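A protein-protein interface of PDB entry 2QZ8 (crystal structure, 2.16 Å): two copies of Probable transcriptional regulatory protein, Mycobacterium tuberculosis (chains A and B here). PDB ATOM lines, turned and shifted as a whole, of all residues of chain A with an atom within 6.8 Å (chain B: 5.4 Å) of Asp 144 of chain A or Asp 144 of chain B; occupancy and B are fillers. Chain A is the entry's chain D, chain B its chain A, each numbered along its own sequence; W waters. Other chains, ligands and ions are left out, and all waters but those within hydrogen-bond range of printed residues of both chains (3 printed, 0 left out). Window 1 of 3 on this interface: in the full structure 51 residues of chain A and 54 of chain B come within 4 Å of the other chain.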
ATOM      1  N   GLN A  51       6.613  13.520   8.942  1.00  0.00           N
ATOM      2  CA  GLN A  51       8.016  13.787   9.218  1.00  0.00           C
ATOM      3  C   GLN A  51       8.573  15.002   8.482  1.00  0.00           C
ATOM      4  O   GLN A  51       9.522  15.634   8.943  1.00  0.00           O
ATOM      5  CB  GLN A  51       8.843  12.533   8.944  1.00  0.00           C
ATOM      6  CG  GLN A  51       8.507  11.406   9.926  1.00  0.00           C
ATOM      7  CD  GLN A  51       9.174  10.073   9.573  1.00  0.00           C
ATOM      8  OE1 GLN A  51       9.585   9.327  10.464  1.00  0.00           O
ATOM      9  NE2 GLN A  51       9.270   9.767   8.275  1.00  0.00           N
ATOM     10  N   SER A  54       9.338  17.728   2.190  1.00  0.00           N
ATOM     11  CA  SER A  54      10.274  17.963   1.096  1.00  0.00           C
ATOM     12  C   SER A  54       9.771  17.344  -0.214  1.00  0.00           C
ATOM     13  O   SER A  54       9.304  16.212  -0.230  1.00  0.00           O
ATOM     14  CB  SER A  54      11.653  17.411   1.462  1.00  0.00           C
ATOM     15  OG  SER A  54      11.522  16.098   1.941  1.00  0.00           O
ATOM     16  N   ARG A  56      10.200  15.393  -3.602  1.00  0.00           N
ATOM     17  CA  ARG A  56      11.172  14.405  -4.077  1.00  0.00           C
ATOM     18  C   ARG A  56      11.899  14.922  -5.314  1.00  0.00           C
ATOM     19  O   ARG A  56      11.279  15.161  -6.342  1.00  0.00           O
ATOM     20  CB  ARG A  56      10.496  13.076  -4.430  1.00  0.00           C
ATOM     21  CG  ARG A  56      10.334  12.070  -3.286  1.00  0.00           C
ATOM     22  CD  ARG A  56      11.456  12.151  -2.268  1.00  0.00           C
ATOM     23  NE  ARG A  56      10.994  12.875  -1.097  1.00  0.00           N
ATOM     24  CZ  ARG A  56      11.723  13.109  -0.015  1.00  0.00           C
ATOM     25  NH1 ARG A  56      12.981  12.674   0.061  1.00  0.00           N
ATOM     26  NH2 ARG A  56      11.183  13.777   0.996  1.00  0.00           N
ATOM     27  N   ILE A  57      13.215  15.088  -5.209  1.00  0.00           N
ATOM     28  CA  ILE A  57      14.037  15.520  -6.339  1.00  0.00           C
ATOM     29  C   ILE A  57      14.867  14.365  -6.917  1.00  0.00           C
ATOM     30  O   ILE A  57      15.472  13.572  -6.165  1.00  0.00           O
ATOM     31  CB  ILE A  57      14.995  16.652  -5.934  1.00  0.00           C
ATOM     32  CG1 ILE A  57      14.239  17.756  -5.172  1.00  0.00           C
ATOM     33  CG2 ILE A  57      15.678  17.226  -7.149  1.00  0.00           C
ATOM     34  CD1 ILE A  57      13.203  18.521  -6.006  1.00  0.00           C
ATOM     35  N   VAL A  93      25.361  11.473   2.594  1.00  0.00           N
ATOM     36  CA  VAL A  93      24.616  10.394   3.238  1.00  0.00           C
ATOM     37  C   VAL A  93      23.133  10.776   3.336  1.00  0.00           C
ATOM     38  O   VAL A  93      22.736  11.649   4.123  1.00  0.00           O
ATOM     39  CB  VAL A  93      25.172  10.056   4.628  1.00  0.00           C
ATOM     40  CG1 VAL A  93      24.454   8.850   5.215  1.00  0.00           C
ATOM     41  CG2 VAL A  93      26.674   9.790   4.554  1.00  0.00           C
ATOM     42  N   GLU A  94      22.322  10.130   2.512  1.00  0.00           N
ATOM     43  CA  GLU A  94      20.893  10.410   2.476  1.00  0.00           C
ATOM     44  C   GLU A  94      20.160   9.710   3.635  1.00  0.00           C
ATOM     45  O   GLU A  94      19.153  10.210   4.149  1.00  0.00           O
ATOM     46  CB  GLU A  94      20.314   9.991   1.114  1.00  0.00           C
ATOM     47  CG  GLU A  94      18.783  10.118   1.020  1.00  0.00           C
ATOM     48  CD  GLU A  94      18.248   9.956  -0.407  1.00  0.00           C
ATOM     49  OE1 GLU A  94      17.174   9.340  -0.577  1.00  0.00           O
ATOM     50  OE2 GLU A  94      18.895  10.442  -1.351  1.00  0.00           O
ATOM     51  N   SER A  95      20.660   8.553   4.057  1.00  0.00           N
ATOM     52  CA  SER A  95      19.981   7.797   5.109  1.00  0.00           C
ATOM     53  C   SER A  95      20.958   6.884   5.810  1.00  0.00           C
ATOM     54  O   SER A  95      21.989   6.519   5.238  1.00  0.00           O
ATOM     55  CB  SER A  95      18.850   6.951   4.514  1.00  0.00           C
ATOM     56  OG  SER A  95      19.411   5.856   3.801  1.00  0.00           O
ATOM     57  N   CYS A  96      20.625   6.486   7.033  1.00  0.00           N
ATOM     58  CA  CYS A  96      21.500   5.604   7.806  1.00  0.00           C
ATOM     59  C   CYS A  96      20.670   4.730   8.731  1.00  0.00           C
ATOM     60  O   CYS A  96      19.834   5.243   9.505  1.00  0.00           O
ATOM     61  CB  CYS A  96      22.508   6.416   8.634  1.00  0.00           C
ATOM     62  SG  CYS A  96      23.529   5.377   9.713  1.00  0.00           S
ATOM     63  N   TYR A  97      20.885   3.417   8.636  1.00  0.00           N
ATOM     64  CA  TYR A  97      20.075   2.431   9.346  1.00  0.00           C
ATOM     65  C   TYR A  97      21.017   1.485  10.055  1.00  0.00           C
ATOM     66  O   TYR A  97      22.046   1.140   9.496  1.00  0.00           O
ATOM     67  CB  TYR A  97      19.240   1.586   8.367  1.00  0.00           C
ATOM     68  CG  TYR A  97      18.438   2.362   7.332  1.00  0.00           C
ATOM     69  CD1 TYR A  97      18.942   2.587   6.058  1.00  0.00           C
ATOM     70  CD2 TYR A  97      17.165   2.847   7.624  1.00  0.00           C
ATOM     71  CE1 TYR A  97      18.209   3.286   5.094  1.00  0.00           C
ATOM     72  CE2 TYR A  97      16.430   3.564   6.676  1.00  0.00           C
ATOM     73  CZ  TYR A  97      16.957   3.775   5.416  1.00  0.00           C
ATOM     74  OH  TYR A  97      16.229   4.475   4.478  1.00  0.00           O
ATOM     75  N   ARG A 110      25.039   9.239  -2.218  1.00  0.00           N
ATOM     76  CA  ARG A 110      24.933   9.844  -3.554  1.00  0.00           C
ATOM     77  C   ARG A 110      26.146  10.717  -3.849  1.00  0.00           C
ATOM     78  O   ARG A 110      26.510  11.586  -3.047  1.00  0.00           O
ATOM     79  CB  ARG A 110      23.716  10.758  -3.622  1.00  0.00           C
ATOM     80  CG  ARG A 110      22.478  10.200  -2.964  1.00  0.00           C
ATOM     81  CD  ARG A 110      21.515   9.745  -4.020  1.00  0.00           C
ATOM     82  NE  ARG A 110      20.217   9.386  -3.468  1.00  0.00           N
ATOM     83  CZ  ARG A 110      19.415   8.486  -4.017  1.00  0.00           C
ATOM     84  NH1 ARG A 110      18.241   8.210  -3.466  1.00  0.00           N
ATOM     85  NH2 ARG A 110      19.793   7.870  -5.125  1.00  0.00           N
ATOM     86  N   TYR A 142      11.774   2.268  -8.875  1.00  0.00           N
ATOM     87  CA  TYR A 142      10.880   3.184  -8.165  1.00  0.00           C
ATOM     88  C   TYR A 142      11.400   3.387  -6.751  1.00  0.00           C
ATOM     89  O   TYR A 142      12.211   2.604  -6.274  1.00  0.00           O
ATOM     90  CB  TYR A 142       9.430   2.681  -8.140  1.00  0.00           C
ATOM     91  CG  TYR A 142       9.268   1.184  -8.039  1.00  0.00           C
ATOM     92  CD1 TYR A 142       9.135   0.553  -6.813  1.00  0.00           C
ATOM     93  CD2 TYR A 142       9.225   0.400  -9.179  1.00  0.00           C
ATOM     94  CE1 TYR A 142       8.991  -0.837  -6.724  1.00  0.00           C
ATOM     95  CE2 TYR A 142       9.085  -0.980  -9.104  1.00  0.00           C
ATOM     96  CZ  TYR A 142       8.962  -1.592  -7.876  1.00  0.00           C
ATOM     97  OH  TYR A 142       8.796  -2.962  -7.815  1.00  0.00           O
ATOM     98  N   SER A 143      10.944   4.424  -6.084  1.00  0.00           N
ATOM     99  CA  SER A 143      11.394   4.624  -4.719  1.00  0.00           C
ATOM    100  C   SER A 143      10.392   5.458  -3.954  1.00  0.00           C
ATOM    101  O   SER A 143       9.651   6.240  -4.585  1.00  0.00           O
ATOM    102  CB  SER A 143      12.782   5.275  -4.730  1.00  0.00           C
ATOM    103  OG  SER A 143      12.836   6.470  -5.467  1.00  0.00           O
ATOM    104  N   ASP A 144      10.548   5.544  -2.650  1.00  0.00           N
ATOM    105  CA  ASP A 144       9.810   6.529  -1.834  1.00  0.00           C
ATOM    106  C   ASP A 144       8.317   6.353  -1.949  1.00  0.00           C
ATOM    107  O   ASP A 144       7.461   7.156  -1.536  1.00  0.00           O
ATOM    108  CB  ASP A 144      10.297   7.931  -2.090  1.00  0.00           C
ATOM    109  CG  ASP A 144      11.685   8.314  -1.725  1.00  0.00           C
ATOM    110  OD1 ASP A 144      12.183   9.304  -2.353  1.00  0.00           O
ATOM    111  OD2 ASP A 144      12.322   7.832  -0.773  1.00  0.00           O
ATOM    112  N   ARG A 145       7.923   5.096  -2.286  1.00  0.00           N
ATOM    113  CA  ARG A 145       6.511   4.758  -2.328  1.00  0.00           C
ATOM    114  C   ARG A 145       5.994   4.369  -0.963  1.00  0.00           C
ATOM    115  O   ARG A 145       6.324   3.347  -0.356  1.00  0.00           O
ATOM    116  CB  ARG A 145       6.181   3.703  -3.364  1.00  0.00           C
ATOM    117  CG  ARG A 145       6.557   3.976  -4.793  1.00  0.00           C
ATOM    118  CD  ARG A 145       6.243   2.819  -5.714  1.00  0.00           C
ATOM    119  NE  ARG A 145       6.200   1.523  -5.023  1.00  0.00           N
ATOM    120  CZ  ARG A 145       5.676   0.441  -5.611  1.00  0.00           C
ATOM    121  NH1 ARG A 145       5.213   0.551  -6.851  1.00  0.00           N
ATOM    122  NH2 ARG A 145       5.599  -0.713  -4.982  1.00  0.00           N
ATOM    123  N   GLN A 146       5.224   5.301  -0.377  1.00  0.00           N
ATOM    124  CA  GLN A 146       4.710   5.025   0.978  1.00  0.00           C
ATOM    125  C   GLN A 146       3.423   4.234   0.869  1.00  0.00           C
ATOM    126  O   GLN A 146       2.664   4.431  -0.103  1.00  0.00           O
ATOM    127  CB  GLN A 146       4.588   6.272   1.816  1.00  0.00           C
ATOM    128  CG  GLN A 146       5.896   7.041   2.032  1.00  0.00           C
ATOM    129  CD  GLN A 146       5.739   8.332   2.786  1.00  0.00           C
ATOM    130  OE1 GLN A 146       6.313   8.563   3.846  1.00  0.00           O
ATOM    131  NE2 GLN A 146       4.979   9.272   2.202  1.00  0.00           N
ATOM    132  N   HIS A 147       3.138   3.410   1.840  1.00  0.00           N
ATOM    133  CA  HIS A 147       1.923   2.573   1.849  1.00  0.00           C
ATOM    134  C   HIS A 147       1.121   2.908   3.077  1.00  0.00           C
ATOM    135  O   HIS A 147       1.450   2.660   4.225  1.00  0.00           O
ATOM    136  CB  HIS A 147       2.240   1.097   1.723  1.00  0.00           C
ATOM    137  CG  HIS A 147       1.088   0.144   1.965  1.00  0.00           C
ATOM    138  ND1 HIS A 147       1.247  -1.006   2.724  1.00  0.00           N
ATOM    139  CD2 HIS A 147      -0.221   0.250   1.680  1.00  0.00           C
ATOM    140  CE1 HIS A 147       0.071  -1.619   2.776  1.00  0.00           C
ATOM    141  NE2 HIS A 147      -0.832  -0.867   2.185  1.00  0.00           N
ATOM    142  N   SER B  54       4.667  13.930  -2.174  1.00  0.00           N
ATOM    143  CA  SER B  54       4.018  13.220  -1.085  1.00  0.00           C
ATOM    144  C   SER B  54       4.663  13.625   0.247  1.00  0.00           C
ATOM    145  O   SER B  54       5.878  13.788   0.325  1.00  0.00           O
ATOM    146  CB  SER B  54       4.136  11.724  -1.306  1.00  0.00           C
ATOM    147  OG  SER B  54       5.433  11.321  -0.953  1.00  0.00           O
ATOM    148  N   ARG B  56       6.169  12.956   3.881  1.00  0.00           N
ATOM    149  CA  ARG B  56       6.839  11.758   4.391  1.00  0.00           C
ATOM    150  C   ARG B  56       6.271  11.331   5.740  1.00  0.00           C
ATOM    151  O   ARG B  56       6.333  12.074   6.714  1.00  0.00           O
ATOM    152  CB  ARG B  56       8.353  11.953   4.483  1.00  0.00           C
ATOM    153  CG  ARG B  56       9.141  10.649   4.342  1.00  0.00           C
ATOM    154  CD  ARG B  56       9.787  10.486   2.954  1.00  0.00           C
ATOM    155  NE  ARG B  56       8.931  10.927   1.855  1.00  0.00           N
ATOM    156  CZ  ARG B  56       8.407  10.121   0.931  1.00  0.00           C
ATOM    157  NH1 ARG B  56       7.645  10.620  -0.028  1.00  0.00           N
ATOM    158  NH2 ARG B  56       8.641   8.817   0.961  1.00  0.00           N
ATOM    159  N   GLU B  94       8.661  -0.180  -1.014  1.00  0.00           N
ATOM    160  CA  GLU B  94       8.792   1.271  -1.087  1.00  0.00           C
ATOM    161  C   GLU B  94       9.725   1.683  -2.211  1.00  0.00           C
ATOM    162  O   GLU B  94       9.523   2.702  -2.875  1.00  0.00           O
ATOM    163  CB  GLU B  94       9.272   1.843   0.249  1.00  0.00           C
ATOM    164  CG  GLU B  94       9.718   3.314   0.171  1.00  0.00           C
ATOM    165  CD  GLU B  94       9.949   3.938   1.545  1.00  0.00           C
ATOM    166  OE1 GLU B  94      10.918   4.708   1.689  1.00  0.00           O
ATOM    167  OE2 GLU B  94       9.168   3.665   2.477  1.00  0.00           O
ATOM    168  N   SER B  95      10.761   0.888  -2.422  1.00  0.00           N
ATOM    169  CA  SER B  95      11.772   1.239  -3.406  1.00  0.00           C
ATOM    170  C   SER B  95      12.390  -0.011  -4.018  1.00  0.00           C
ATOM    171  O   SER B  95      12.433  -1.071  -3.402  1.00  0.00           O
ATOM    172  CB  SER B  95      12.856   2.108  -2.754  1.00  0.00           C
ATOM    173  OG  SER B  95      13.611   1.308  -1.855  1.00  0.00           O
ATOM    174  N   TYR B 142      18.464   8.354  10.496  1.00  0.00           N
ATOM    175  CA  TYR B 142      17.977   9.450   9.691  1.00  0.00           C
ATOM    176  C   TYR B 142      17.791   8.954   8.268  1.00  0.00           C
ATOM    177  O   TYR B 142      18.424   7.998   7.850  1.00  0.00           O
ATOM    178  CB  TYR B 142      18.901  10.668   9.755  1.00  0.00           C
ATOM    179  CG  TYR B 142      20.382  10.373   9.724  1.00  0.00           C
ATOM    180  CD1 TYR B 142      21.066  10.255   8.520  1.00  0.00           C
ATOM    181  CD2 TYR B 142      21.108  10.257  10.903  1.00  0.00           C
ATOM    182  CE1 TYR B 142      22.422   9.998   8.493  1.00  0.00           C
ATOM    183  CE2 TYR B 142      22.458  10.000  10.884  1.00  0.00           C
ATOM    184  CZ  TYR B 142      23.112   9.868   9.678  1.00  0.00           C
ATOM    185  OH  TYR B 142      24.470   9.619   9.664  1.00  0.00           O
ATOM    186  N   SER B 143      16.893   9.578   7.531  1.00  0.00           N
ATOM    187  CA  SER B 143      16.626   9.118   6.176  1.00  0.00           C
ATOM    188  C   SER B 143      16.074  10.247   5.341  1.00  0.00           C
ATOM    189  O   SER B 143      15.803  11.342   5.853  1.00  0.00           O
ATOM    190  CB  SER B 143      15.660   7.925   6.172  1.00  0.00           C
ATOM    191  OG  SER B 143      14.451   8.258   6.833  1.00  0.00           O
ATOM    192  N   ASP B 144      15.943   9.963   4.050  1.00  0.00           N
ATOM    193  CA  ASP B 144      15.478  10.915   3.048  1.00  0.00           C
ATOM    194  C   ASP B 144      16.098  12.298   3.152  1.00  0.00           C
ATOM    195  O   ASP B 144      15.407  13.300   2.954  1.00  0.00           O
ATOM    196  CB  ASP B 144      13.946  11.001   3.040  1.00  0.00           C
ATOM    197  CG  ASP B 144      13.289   9.645   2.748  1.00  0.00           C
ATOM    198  OD1 ASP B 144      12.434   9.202   3.547  1.00  0.00           O
ATOM    199  OD2 ASP B 144      13.659   9.003   1.735  1.00  0.00           O
ATOM    200  N   ARG B 145      17.395  12.358   3.431  1.00  0.00           N
ATOM    201  CA  ARG B 145      18.096  13.645   3.451  1.00  0.00           C
ATOM    202  C   ARG B 145      18.663  14.040   2.085  1.00  0.00           C
ATOM    203  O   ARG B 145      19.828  13.772   1.773  1.00  0.00           O
ATOM    204  CB  ARG B 145      19.217  13.637   4.493  1.00  0.00           C
ATOM    205  CG  ARG B 145      18.771  13.199   5.873  1.00  0.00           C
ATOM    206  CD  ARG B 145      19.861  13.434   6.882  1.00  0.00           C
ATOM    207  NE  ARG B 145      21.165  13.022   6.366  1.00  0.00           N
ATOM    208  CZ  ARG B 145      22.314  13.270   6.984  1.00  0.00           C
ATOM    209  NH1 ARG B 145      22.295  13.917   8.142  1.00  0.00           N
ATOM    210  NH2 ARG B 145      23.474  12.880   6.450  1.00  0.00           N
ATOM    211  N   GLN B 146      17.855  14.723   1.286  1.00  0.00           N
ATOM    212  CA  GLN B 146      18.260  15.085  -0.065  1.00  0.00           C
ATOM    213  C   GLN B 146      19.284  16.214  -0.116  1.00  0.00           C
ATOM    214  O   GLN B 146      19.036  17.326   0.348  1.00  0.00           O
ATOM    215  CB  GLN B 146      17.042  15.472  -0.892  1.00  0.00           C
ATOM    216  CG  GLN B 146      16.101  14.326  -1.156  1.00  0.00           C
ATOM    217  CD  GLN B 146      14.829  14.802  -1.806  1.00  0.00           C
ATOM    218  OE1 GLN B 146      14.369  14.238  -2.803  1.00  0.00           O
ATOM    219  NE2 GLN B 146      14.256  15.866  -1.253  1.00  0.00           N
HETATM  220  O   HOH W   1       8.192  14.574   1.838  1.00  0.00           O
HETATM  221  O   HOH W   2      16.429   7.560   1.749  1.00  0.00           O
HETATM  222  O   HOH W   3       7.725  14.215  -1.383  1.00  0.00           O
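Among the printed residues, merely in contact across the chains: Arg 56 of chain A with Arg 56 of chain B (3.7 Å), Arg 56 of chain A with Asp 144 of chain B (3.6 Å), Arg 56 of chain A with Gln 146 of chain B (3.4 Å), Glu 94 of chain A with Ser 143 of chain B (3.3 Å), Ser 95 of chain A with Tyr 142 of chain B (3.2 Å), Ser 95 of chain A with Ser 143 of chain B (3.5 Å), Tyr 97 of chain A with Ser 143 of chain B (3.9 Å), Tyr 142 of chain A with Ser 95 of chain B (3.2 Å), Ser 143 of chain A with Glu 94 of chain B (3.1 Å), Ser 143 of chain A with Ser 95 of chain B (3.5 Å), Gln 146 of chain A with Ser 54 of chain B (3.8 Å) and Gln 146 of chain A with Arg 56 of chain B (3.3 Å).
O of Arg 56 of chain B lies within hydrogen-bond range of N of Gln 51 of chain A (2.7 Å).
The backbone carbonyl oxygen (O) of Asp 144 of chain A sits at hydrogen-bond distance from the guanidinium group (NH2) of Arg 56 of chain B (3.2 Å).
N of Asp 144 of chain A is in hydrogen-bond range of O of Glu 94 of chain B, at 3.0 Å.
O of Glu 94 of chain B lies within hydrogen-bond range of N of Arg 145 of chain A.
N of Cys 96 of chain A is in hydrogen-bond range of O of Tyr 142 of chain B (2.8 Å).
The backbone carbonyl oxygen (O) of Glu 94 of chain A is in hydrogen-bond range of the backbone NH (N) of Asp 144 of chain B (3.2 Å).
The backbone carbonyl oxygen of Val 93 of chain A is in hydrogen-bond range of the guanidinium group of Arg 145 of chain B, 2.7 Å away.
O of Glu 94 of chain A sits at hydrogen-bond distance from N of Arg 145 of chain B (2.9 Å).
The side-chain amide oxygen of Gln 146 of chain B lies within hydrogen-bond range of the backbone NH of Ile 57 of chain A.
The side-chain carboxylate (OD2) of Asp 144 of chain A lies close to the side-chain carboxylate (OD2) of Asp 144 of chain B (3.1 Å).
Of the 9 printed residues of chain B, 9 touch a printed residue of chain A.
Printed residues of chain B that touch a printed residue of chain A: Ser 54, Arg 56, Glu 94, Ser 95, Tyr 142, Ser 143, Asp 144, Arg 145 and Gln 146.
Hydrophobic or aromatic side chains of chain B that line the printed part of chain A: Tyr 142.
Hydrophobic or aromatic side chains of chain A within 4 Å of the printed part of chain B: Val 93 and Tyr 97.
Along chain A the printed residues that touch a printed residue of chain B span positions 51 to 146.
Among the printed residues, no Asp or Glu carboxylate lies within 4 Å of a Lys or Arg side-chain nitrogen of the other chain.
Glu 94 of chain A touches Ser 143 of chain B, and with the chains exchanged Ser 143 of chain A touches Glu 94 of chain B.
Glu 94 of chain A touches Asp 144 of chain B, and with the chains exchanged Asp 144 of chain A touches Glu 94 of chain B.
Ser 95 of chain A touches Tyr 142 of chain B, and with the chains exchanged Tyr 142 of chain A touches Ser 95 of chain B.
Ser 95 of chain A touches Ser 143 of chain B, and with the chains exchanged Ser 143 of chain A touches Ser 95 of chain B.
9 positions are printed for both chains.
Of the 22 pairs that touch across the chains among the printed residues, 16 have their exchanged pair printed and touching as well.
NH1 of Arg 56 of chain B is in hydrogen-bond range of OG of Ser 54 of chain B (2.5 Å).
OG of Ser 54 of chain A lies within hydrogen-bond range of NH2 of Arg 56 of chain A.
The side-chain carboxylate (OD1) of Asp 144 of chain A is in salt-bridge range of the guanidinium group (NE) of Arg 56 of chain A (3.97 Å).
OE2 of Glu 94 of chain A is in salt-bridge range of NE of Arg 110 of chain A (2.7 Å).
Asp 144 of chain A touches just these residues of chain B: Arg 56 (3.2 Å), Glu 94 (3.0 Å) and Asp 144 (3.1 Å).
Asp 144 of chain B touches just these residues of chain A: Arg 56 (3.6 Å), Glu 94 (3.2 Å) and Asp 144 (3.1 Å).
Of the printed residues of chain B, Tyr 97 of chain A touches Ser 143 (3.9 Å).
Of the printed residues of chain A, Tyr 142 of chain B touches Ser 95 and Cys 96.
Of the printed residues of chain A, Arg 145 of chain B touches Val 93 and Glu 94.
Printed residues of chain A within 4 Å of Ser 143 of chain B: Glu 94 (3.3 Å), Ser 95 (3.5 Å) and Tyr 97 (3.9 Å).
Ser 54 of chain A touches none of the printed residues of chain B.
The nearest printed residue of chain B that does not touch Ser 95 of chain A is Asp 144 of chain B (4.2 Å).
Water W3 lies within hydrogen-bond range of O of Ser 54 of chain B (2.6 Å) and O of Ser 54 of chain A (2.8 Å).
Water W1 lies within hydrogen-bond range of O of Ser 54 of chain A (2.9 Å), O of Ser 54 of chain B (2.9 Å), NH2 of Arg 56 of chain A (3.2 Å) and N of Arg 56 of chain B (3.3 Å).
Water W2 bridges the side-chain carboxylate (OE1) of Glu 94 of chain A and the side-chain carboxylate (OD2) of Asp 144 of chain B.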
